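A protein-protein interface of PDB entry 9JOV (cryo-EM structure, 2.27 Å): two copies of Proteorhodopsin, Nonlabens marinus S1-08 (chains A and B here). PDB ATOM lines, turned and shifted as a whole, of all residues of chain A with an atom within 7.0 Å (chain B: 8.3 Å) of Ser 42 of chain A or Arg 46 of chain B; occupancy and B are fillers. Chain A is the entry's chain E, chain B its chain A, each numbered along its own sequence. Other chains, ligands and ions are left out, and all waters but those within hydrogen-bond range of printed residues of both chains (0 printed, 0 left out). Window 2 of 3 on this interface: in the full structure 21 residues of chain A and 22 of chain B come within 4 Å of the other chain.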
ATOM      1  N   PHE A  37      19.226 -21.617  18.957  1.00  0.00           N
ATOM      2  CA  PHE A  37      19.314 -20.742  17.789  1.00  0.00           C
ATOM      3  C   PHE A  37      20.779 -20.482  17.431  1.00  0.00           C
ATOM      4  O   PHE A  37      21.184 -20.654  16.292  1.00  0.00           O
ATOM      5  CB  PHE A  37      18.561 -19.431  18.007  1.00  0.00           C
ATOM      6  CG  PHE A  37      17.066 -19.557  18.248  1.00  0.00           C
ATOM      7  CD1 PHE A  37      16.271 -20.237  17.336  1.00  0.00           C
ATOM      8  CD2 PHE A  37      16.456 -18.984  19.370  1.00  0.00           C
ATOM      9  CE1 PHE A  37      14.902 -20.368  17.540  1.00  0.00           C
ATOM     10  CE2 PHE A  37      15.094 -19.141  19.584  1.00  0.00           C
ATOM     11  CZ  PHE A  37      14.314 -19.812  18.650  1.00  0.00           C
ATOM     12  N   PHE A  38      21.629 -20.127  18.404  1.00  0.00           N
ATOM     13  CA  PHE A  38      23.043 -19.954  18.065  1.00  0.00           C
ATOM     14  C   PHE A  38      23.675 -21.201  17.443  1.00  0.00           C
ATOM     15  O   PHE A  38      24.429 -21.082  16.491  1.00  0.00           O
ATOM     16  CB  PHE A  38      23.908 -19.615  19.272  1.00  0.00           C
ATOM     17  CG  PHE A  38      23.568 -18.257  19.867  1.00  0.00           C
ATOM     18  CD1 PHE A  38      23.073 -17.231  19.044  1.00  0.00           C
ATOM     19  CD2 PHE A  38      23.704 -18.013  21.222  1.00  0.00           C
ATOM     20  CE1 PHE A  38      22.754 -16.000  19.559  1.00  0.00           C
ATOM     21  CE2 PHE A  38      23.432 -16.745  21.731  1.00  0.00           C
ATOM     22  CZ  PHE A  38      22.929 -15.749  20.904  1.00  0.00           C
ATOM     23  N   LEU A  39      23.363 -22.403  17.958  1.00  0.00           N
ATOM     24  CA  LEU A  39      24.013 -23.610  17.466  1.00  0.00           C
ATOM     25  C   LEU A  39      23.385 -24.088  16.159  1.00  0.00           C
ATOM     26  O   LEU A  39      24.012 -24.861  15.469  1.00  0.00           O
ATOM     27  CB  LEU A  39      24.016 -24.697  18.527  1.00  0.00           C
ATOM     28  CG  LEU A  39      24.914 -24.401  19.745  1.00  0.00           C
ATOM     29  CD1 LEU A  39      24.782 -25.351  20.903  1.00  0.00           C
ATOM     30  CD2 LEU A  39      26.335 -24.401  19.315  1.00  0.00           C
ATOM     31  N   SER A  40      22.186 -23.613  15.787  1.00  0.00           N
ATOM     32  CA  SER A  40      21.557 -24.083  14.568  1.00  0.00           C
ATOM     33  C   SER A  40      22.014 -23.261  13.378  1.00  0.00           C
ATOM     34  O   SER A  40      21.832 -23.699  12.233  1.00  0.00           O
ATOM     35  CB  SER A  40      20.065 -24.029  14.632  1.00  0.00           C
ATOM     36  OG  SER A  40      19.533 -24.642  15.793  1.00  0.00           O
ATOM     37  N   MET A  41      22.518 -22.046  13.630  1.00  0.00           N
ATOM     38  CA  MET A  41      22.730 -21.050  12.579  1.00  0.00           C
ATOM     39  C   MET A  41      23.545 -21.635  11.422  1.00  0.00           C
ATOM     40  O   MET A  41      23.213 -21.409  10.253  1.00  0.00           O
ATOM     41  CB  MET A  41      23.587 -19.908  13.098  1.00  0.00           C
ATOM     42  CG  MET A  41      22.916 -18.761  13.722  1.00  0.00           C
ATOM     43  SD  MET A  41      24.270 -17.680  14.254  1.00  0.00           S
ATOM     44  CE  MET A  41      24.716 -17.122  12.611  1.00  0.00           C
ATOM     45  N   SER A  42      24.589 -22.425  11.745  1.00  0.00           N
ATOM     46  CA  SER A  42      25.521 -22.902  10.723  1.00  0.00           C
ATOM     47  C   SER A  42      24.958 -23.996   9.805  1.00  0.00           C
ATOM     48  O   SER A  42      25.612 -24.378   8.848  1.00  0.00           O
ATOM     49  CB  SER A  42      26.753 -23.419  11.367  1.00  0.00           C
ATOM     50  OG  SER A  42      26.501 -24.712  11.898  1.00  0.00           O
ATOM     51  N   SER A  43      23.764 -24.525  10.090  1.00  0.00           N
ATOM     52  CA  SER A  43      23.198 -25.582   9.272  1.00  0.00           C
ATOM     53  C   SER A  43      22.293 -25.000   8.184  1.00  0.00           C
ATOM     54  O   SER A  43      21.482 -25.714   7.597  1.00  0.00           O
ATOM     55  CB  SER A  43      22.419 -26.530  10.136  1.00  0.00           C
ATOM     56  OG  SER A  43      23.232 -27.091  11.156  1.00  0.00           O
ATOM     57  N   PHE A  44      22.394 -23.697   7.951  1.00  0.00           N
ATOM     58  CA  PHE A  44      21.550 -22.997   7.003  1.00  0.00           C
ATOM     59  C   PHE A  44      22.439 -22.187   6.060  1.00  0.00           C
ATOM     60  O   PHE A  44      23.523 -21.725   6.425  1.00  0.00           O
ATOM     61  CB  PHE A  44      20.614 -21.959   7.641  1.00  0.00           C
ATOM     62  CG  PHE A  44      19.463 -22.533   8.435  1.00  0.00           C
ATOM     63  CD1 PHE A  44      18.375 -23.066   7.777  1.00  0.00           C
ATOM     64  CD2 PHE A  44      19.476 -22.570   9.828  1.00  0.00           C
ATOM     65  CE1 PHE A  44      17.334 -23.648   8.485  1.00  0.00           C
ATOM     66  CE2 PHE A  44      18.421 -23.159  10.533  1.00  0.00           C
ATOM     67  CZ  PHE A  44      17.359 -23.693   9.861  1.00  0.00           C
ATOM     68  N   GLU A  45      21.926 -21.977   4.849  1.00  0.00           N
ATOM     69  CA  GLU A  45      22.557 -21.099   3.891  1.00  0.00           C
ATOM     70  C   GLU A  45      22.659 -19.711   4.525  1.00  0.00           C
ATOM     71  O   GLU A  45      21.778 -19.321   5.293  1.00  0.00           O
ATOM     72  CB  GLU A  45      21.709 -20.980   2.621  1.00  0.00           C
ATOM     73  CG  GLU A  45      21.307 -22.296   1.967  1.00  0.00           C
ATOM     74  CD  GLU A  45      20.345 -22.070   0.810  1.00  0.00           C
ATOM     75  OE1 GLU A  45      19.167 -22.488   0.929  1.00  0.00           O
ATOM     76  OE2 GLU A  45      20.759 -21.470  -0.213  1.00  0.00           O
ATOM     77  N   ARG A  49      20.817 -16.975   7.958  1.00  0.00           N
ATOM     78  CA  ARG A  49      21.538 -16.976   9.211  1.00  0.00           C
ATOM     79  C   ARG A  49      21.244 -15.754  10.081  1.00  0.00           C
ATOM     80  O   ARG A  49      21.133 -15.887  11.302  1.00  0.00           O
ATOM     81  CB  ARG A  49      23.040 -17.050   8.955  1.00  0.00           C
ATOM     82  CG  ARG A  49      23.364 -18.449   8.514  1.00  0.00           C
ATOM     83  CD  ARG A  49      24.880 -18.591   8.544  1.00  0.00           C
ATOM     84  NE  ARG A  49      25.112 -19.847   7.813  1.00  0.00           N
ATOM     85  CZ  ARG A  49      26.263 -20.190   7.340  1.00  0.00           C
ATOM     86  NH1 ARG A  49      27.323 -19.498   7.735  1.00  0.00           N
ATOM     87  NH2 ARG A  49      26.355 -21.256   6.553  1.00  0.00           N
ATOM     88  N   ILE A  52      18.105 -15.918  12.117  1.00  0.00           N
ATOM     89  CA  ILE A  52      18.199 -16.855  13.218  1.00  0.00           C
ATOM     90  C   ILE A  52      19.074 -16.287  14.331  1.00  0.00           C
ATOM     91  O   ILE A  52      18.692 -16.319  15.513  1.00  0.00           O
ATOM     92  CB  ILE A  52      18.629 -18.239  12.711  1.00  0.00           C
ATOM     93  CG1 ILE A  52      17.535 -18.816  11.850  1.00  0.00           C
ATOM     94  CG2 ILE A  52      18.987 -19.150  13.885  1.00  0.00           C
ATOM     95  CD1 ILE A  52      18.026 -19.916  10.970  1.00  0.00           C
ATOM     96  N   THR A 238      14.395 -24.148   3.099  1.00  0.00           N
ATOM     97  CA  THR A 238      15.572 -24.948   2.825  1.00  0.00           C
ATOM     98  C   THR A 238      15.188 -26.303   2.246  1.00  0.00           C
ATOM     99  O   THR A 238      15.909 -26.835   1.408  1.00  0.00           O
ATOM    100  CB  THR A 238      16.334 -25.124   4.137  1.00  0.00           C
ATOM    101  OG1 THR A 238      16.919 -23.862   4.431  1.00  0.00           O
ATOM    102  CG2 THR A 238      17.402 -26.194   4.021  1.00  0.00           C
ATOM    103  N   MET B  41      28.319 -32.149  16.908  1.00  0.00           N
ATOM    104  CA  MET B  41      27.280 -31.869  15.929  1.00  0.00           C
ATOM    105  C   MET B  41      27.869 -31.698  14.526  1.00  0.00           C
ATOM    106  O   MET B  41      27.341 -32.219  13.547  1.00  0.00           O
ATOM    107  CB  MET B  41      26.590 -30.551  16.243  1.00  0.00           C
ATOM    108  CG  MET B  41      25.431 -30.595  17.175  1.00  0.00           C
ATOM    109  SD  MET B  41      24.978 -28.852  17.399  1.00  0.00           S
ATOM    110  CE  MET B  41      24.266 -28.615  15.775  1.00  0.00           C
ATOM    111  N   SER B  42      28.985 -30.971  14.430  1.00  0.00           N
ATOM    112  CA  SER B  42      29.541 -30.569  13.144  1.00  0.00           C
ATOM    113  C   SER B  42      30.221 -31.711  12.374  1.00  0.00           C
ATOM    114  O   SER B  42      30.661 -31.520  11.252  1.00  0.00           O
ATOM    115  CB  SER B  42      30.536 -29.472  13.355  1.00  0.00           C
ATOM    116  OG  SER B  42      31.753 -30.032  13.842  1.00  0.00           O
ATOM    117  N   SER B  43      30.367 -32.891  12.971  1.00  0.00           N
ATOM    118  CA  SER B  43      31.008 -34.009  12.306  1.00  0.00           C
ATOM    119  C   SER B  43      29.984 -34.868  11.556  1.00  0.00           C
ATOM    120  O   SER B  43      30.283 -35.993  11.184  1.00  0.00           O
ATOM    121  CB  SER B  43      31.743 -34.830  13.317  1.00  0.00           C
ATOM    122  OG  SER B  43      32.742 -34.048  13.962  1.00  0.00           O
ATOM    123  N   PHE B  44      28.756 -34.367  11.419  1.00  0.00           N
ATOM    124  CA  PHE B  44      27.649 -35.133  10.878  1.00  0.00           C
ATOM    125  C   PHE B  44      26.995 -34.332   9.759  1.00  0.00           C
ATOM    126  O   PHE B  44      26.995 -33.102   9.774  1.00  0.00           O
ATOM    127  CB  PHE B  44      26.529 -35.426  11.877  1.00  0.00           C
ATOM    128  CG  PHE B  44      26.876 -36.468  12.924  1.00  0.00           C
ATOM    129  CD1 PHE B  44      26.915 -37.815  12.587  1.00  0.00           C
ATOM    130  CD2 PHE B  44      27.171 -36.105  14.242  1.00  0.00           C
ATOM    131  CE1 PHE B  44      27.255 -38.779  13.537  1.00  0.00           C
ATOM    132  CE2 PHE B  44      27.509 -37.078  15.184  1.00  0.00           C
ATOM    133  CZ  PHE B  44      27.558 -38.407  14.834  1.00  0.00           C
ATOM    134  N   GLU B  45      26.418 -35.045   8.794  1.00  0.00           N
ATOM    135  CA  GLU B  45      25.620 -34.416   7.762  1.00  0.00           C
ATOM    136  C   GLU B  45      24.471 -33.669   8.440  1.00  0.00           C
ATOM    137  O   GLU B  45      23.979 -34.119   9.471  1.00  0.00           O
ATOM    138  CB  GLU B  45      25.017 -35.448   6.816  1.00  0.00           C
ATOM    139  CG  GLU B  45      25.985 -36.452   6.210  1.00  0.00           C
ATOM    140  CD  GLU B  45      25.239 -37.597   5.538  1.00  0.00           C
ATOM    141  OE1 GLU B  45      25.388 -38.744   6.017  1.00  0.00           O
ATOM    142  OE2 GLU B  45      24.505 -37.351   4.549  1.00  0.00           O
ATOM    143  N   ARG B  46      24.010 -32.582   7.805  1.00  0.00           N
ATOM    144  CA  ARG B  46      22.970 -31.718   8.337  1.00  0.00           C
ATOM    145  C   ARG B  46      21.756 -32.496   8.829  1.00  0.00           C
ATOM    146  O   ARG B  46      21.186 -32.125   9.850  1.00  0.00           O
ATOM    147  CB  ARG B  46      22.574 -30.630   7.338  1.00  0.00           C
ATOM    148  CG  ARG B  46      23.624 -29.524   7.320  1.00  0.00           C
ATOM    149  CD  ARG B  46      23.582 -28.654   6.064  1.00  0.00           C
ATOM    150  NE  ARG B  46      24.645 -27.642   6.107  1.00  0.00           N
ATOM    151  CZ  ARG B  46      24.565 -26.391   5.648  1.00  0.00           C
ATOM    152  NH1 ARG B  46      23.513 -25.973   4.957  1.00  0.00           N
ATOM    153  NH2 ARG B  46      25.570 -25.552   5.842  1.00  0.00           N
ATOM    154  N   LYS B  47      21.375 -33.568   8.149  1.00  0.00           N
ATOM    155  CA  LYS B  47      20.150 -34.287   8.496  1.00  0.00           C
ATOM    156  C   LYS B  47      20.164 -34.890   9.908  1.00  0.00           C
ATOM    157  O   LYS B  47      19.122 -35.269  10.407  1.00  0.00           O
ATOM    158  CB  LYS B  47      19.875 -35.405   7.478  1.00  0.00           C
ATOM    159  CG  LYS B  47      20.518 -36.742   7.775  1.00  0.00           C
ATOM    160  CD  LYS B  47      20.079 -37.860   6.842  1.00  0.00           C
ATOM    161  CE  LYS B  47      20.638 -37.777   5.461  1.00  0.00           C
ATOM    162  NZ  LYS B  47      20.104 -38.861   4.632  1.00  0.00           N
ATOM    163  N   TRP B  48      21.326 -35.069  10.537  1.00  0.00           N
ATOM    164  CA  TRP B  48      21.360 -35.633  11.871  1.00  0.00           C
ATOM    165  C   TRP B  48      21.521 -34.552  12.939  1.00  0.00           C
ATOM    166  O   TRP B  48      21.304 -34.799  14.134  1.00  0.00           O
ATOM    167  CB  TRP B  48      22.503 -36.652  12.021  1.00  0.00           C
ATOM    168  CG  TRP B  48      22.473 -37.719  10.969  1.00  0.00           C
ATOM    169  CD1 TRP B  48      23.215 -37.800   9.827  1.00  0.00           C
ATOM    170  CD2 TRP B  48      21.599 -38.857  10.968  1.00  0.00           C
ATOM    171  NE1 TRP B  48      22.863 -38.910   9.113  1.00  0.00           N
ATOM    172  CE2 TRP B  48      21.886 -39.582   9.796  1.00  0.00           C
ATOM    173  CE3 TRP B  48      20.639 -39.337  11.852  1.00  0.00           C
ATOM    174  CZ2 TRP B  48      21.216 -40.753   9.475  1.00  0.00           C
ATOM    175  CZ3 TRP B  48      19.998 -40.513  11.549  1.00  0.00           C
ATOM    176  CH2 TRP B  48      20.275 -41.201  10.373  1.00  0.00           C
ATOM    177  N   ARG B  49      22.032 -33.404  12.543  1.00  0.00           N
ATOM    178  CA  ARG B  49      22.507 -32.436  13.508  1.00  0.00           C
ATOM    179  C   ARG B  49      21.435 -32.004  14.513  1.00  0.00           C
ATOM    180  O   ARG B  49      21.747 -31.807  15.697  1.00  0.00           O
ATOM    181  CB  ARG B  49      23.034 -31.210  12.781  1.00  0.00           C
ATOM    182  CG  ARG B  49      24.321 -31.565  12.095  1.00  0.00           C
ATOM    183  CD  ARG B  49      24.926 -30.225  11.605  1.00  0.00           C
ATOM    184  NE  ARG B  49      26.074 -30.641  10.795  1.00  0.00           N
ATOM    185  CZ  ARG B  49      26.675 -29.871   9.954  1.00  0.00           C
ATOM    186  NH1 ARG B  49      26.310 -28.593   9.931  1.00  0.00           N
ATOM    187  NH2 ARG B  49      27.604 -30.381   9.150  1.00  0.00           N
ATOM    188  N   THR B  50      20.169 -31.872  14.098  1.00  0.00           N
ATOM    189  CA  THR B  50      19.160 -31.371  15.034  1.00  0.00           C
ATOM    190  C   THR B  50      18.905 -32.376  16.156  1.00  0.00           C
ATOM    191  O   THR B  50      18.791 -31.969  17.304  1.00  0.00           O
ATOM    192  CB  THR B  50      17.838 -31.066  14.336  1.00  0.00           C
ATOM    193  OG1 THR B  50      18.105 -30.113  13.326  1.00  0.00           O
ATOM    194  CG2 THR B  50      16.861 -30.393  15.262  1.00  0.00           C
ATOM    195  N   SER B  51      18.786 -33.671  15.838  1.00  0.00           N
ATOM    196  CA  SER B  51      18.583 -34.657  16.876  1.00  0.00           C
ATOM    197  C   SER B  51      19.753 -34.618  17.884  1.00  0.00           C
ATOM    198  O   SER B  51      19.539 -34.761  19.101  1.00  0.00           O
ATOM    199  CB  SER B  51      18.434 -36.018  16.296  1.00  0.00           C
ATOM    200  OG  SER B  51      19.669 -36.431  15.703  1.00  0.00           O
ATOM    201  N   ILE B  52      20.974 -34.344  17.409  1.00  0.00           N
ATOM    202  CA  ILE B  52      22.083 -34.290  18.355  1.00  0.00           C
ATOM    203  C   ILE B  52      22.045 -32.999  19.178  1.00  0.00           C
ATOM    204  O   ILE B  52      22.148 -33.043  20.402  1.00  0.00           O
ATOM    205  CB  ILE B  52      23.403 -34.541  17.627  1.00  0.00           C
ATOM    206  CG1 ILE B  52      23.424 -36.001  17.115  1.00  0.00           C
ATOM    207  CG2 ILE B  52      24.582 -34.226  18.523  1.00  0.00           C
ATOM    208  CD1 ILE B  52      24.448 -36.181  16.021  1.00  0.00           C
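The guanidinium group (NH2) of Arg 46 of chain B lies within hydrogen-bond range of the backbone carbonyl oxygen (O) of Ser 42 of chain A (3.2 Å).
The guanidinium group (NH1) of Arg 46 of chain B is in hydrogen-bond range of the backbone carbonyl oxygen (O) of Ser 43 of chain A (3.3 Å).
The backbone carbonyl oxygen (O) of Phe 44 of chain A sits at hydrogen-bond distance from the guanidinium group (NE) of Arg 49 of chain A (2.8 Å).
The backbone carbonyl oxygen (O) of Met 41 of chain B lies close to the guanidinium group (NE) of Arg 49 of chain B (3.4 Å).
The backbone carbonyl oxygen (O) of Phe 44 of chain B lies within hydrogen-bond range of the guanidinium group (NE) of Arg 49 of chain B, at 2.8 Å.
Among the printed residues, pairs that only touch across the chains: Ser 43 of chain A with Arg 49 of chain B, Leu 39 of chain A with Met 41 of chain B and Phe 44 of chain A with Arg 46 of chain B.
Of chain B, only Arg 46 (3.2 Å) comes within 4 Å of Ser 42 of chain A.
Arg 46 of chain B touches three residues of chain A.
Of chain B, only Arg 46 (3.3 Å) and Arg 49 (3.6 Å) come within 4 Å of Ser 43 of chain A.
Of the printed residues of chain B, Leu 39 of chain A touches Met 41 (3.8 Å).
Of the printed residues of chain A, Met 41 of chain B touches Leu 39 (3.8 Å).
Trp 48 of chain B touches none of the printed residues of chain A.
Ser 42 of chain B touches none of the printed residues of chain A.
The nearest residue of chain A that does not touch Arg 46 of chain B is Glu 45 of chain A (4.3 Å).
Hydrophobic or aromatic side chains of chain B within 4 Å of the printed part of chain A: Met 41.
Along chain B the printed residues that touch a printed residue of chain A span positions 41 to 49.
Among the printed residues, 5 pairs touch across the chains.
Among the printed residues, no Asp or Glu carboxylate lies within 4 Å of a Lys or Arg side-chain nitrogen of the other chain.
Ser 43 of chain A touches Arg 49 of chain B, but with the chains exchanged Arg 49 of chain A does not touch Ser 43 of chain B (13.9 Å).
Of the 5 pairs that touch across the chains among the printed residues, none has its exchanged pair printed and touching as well.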
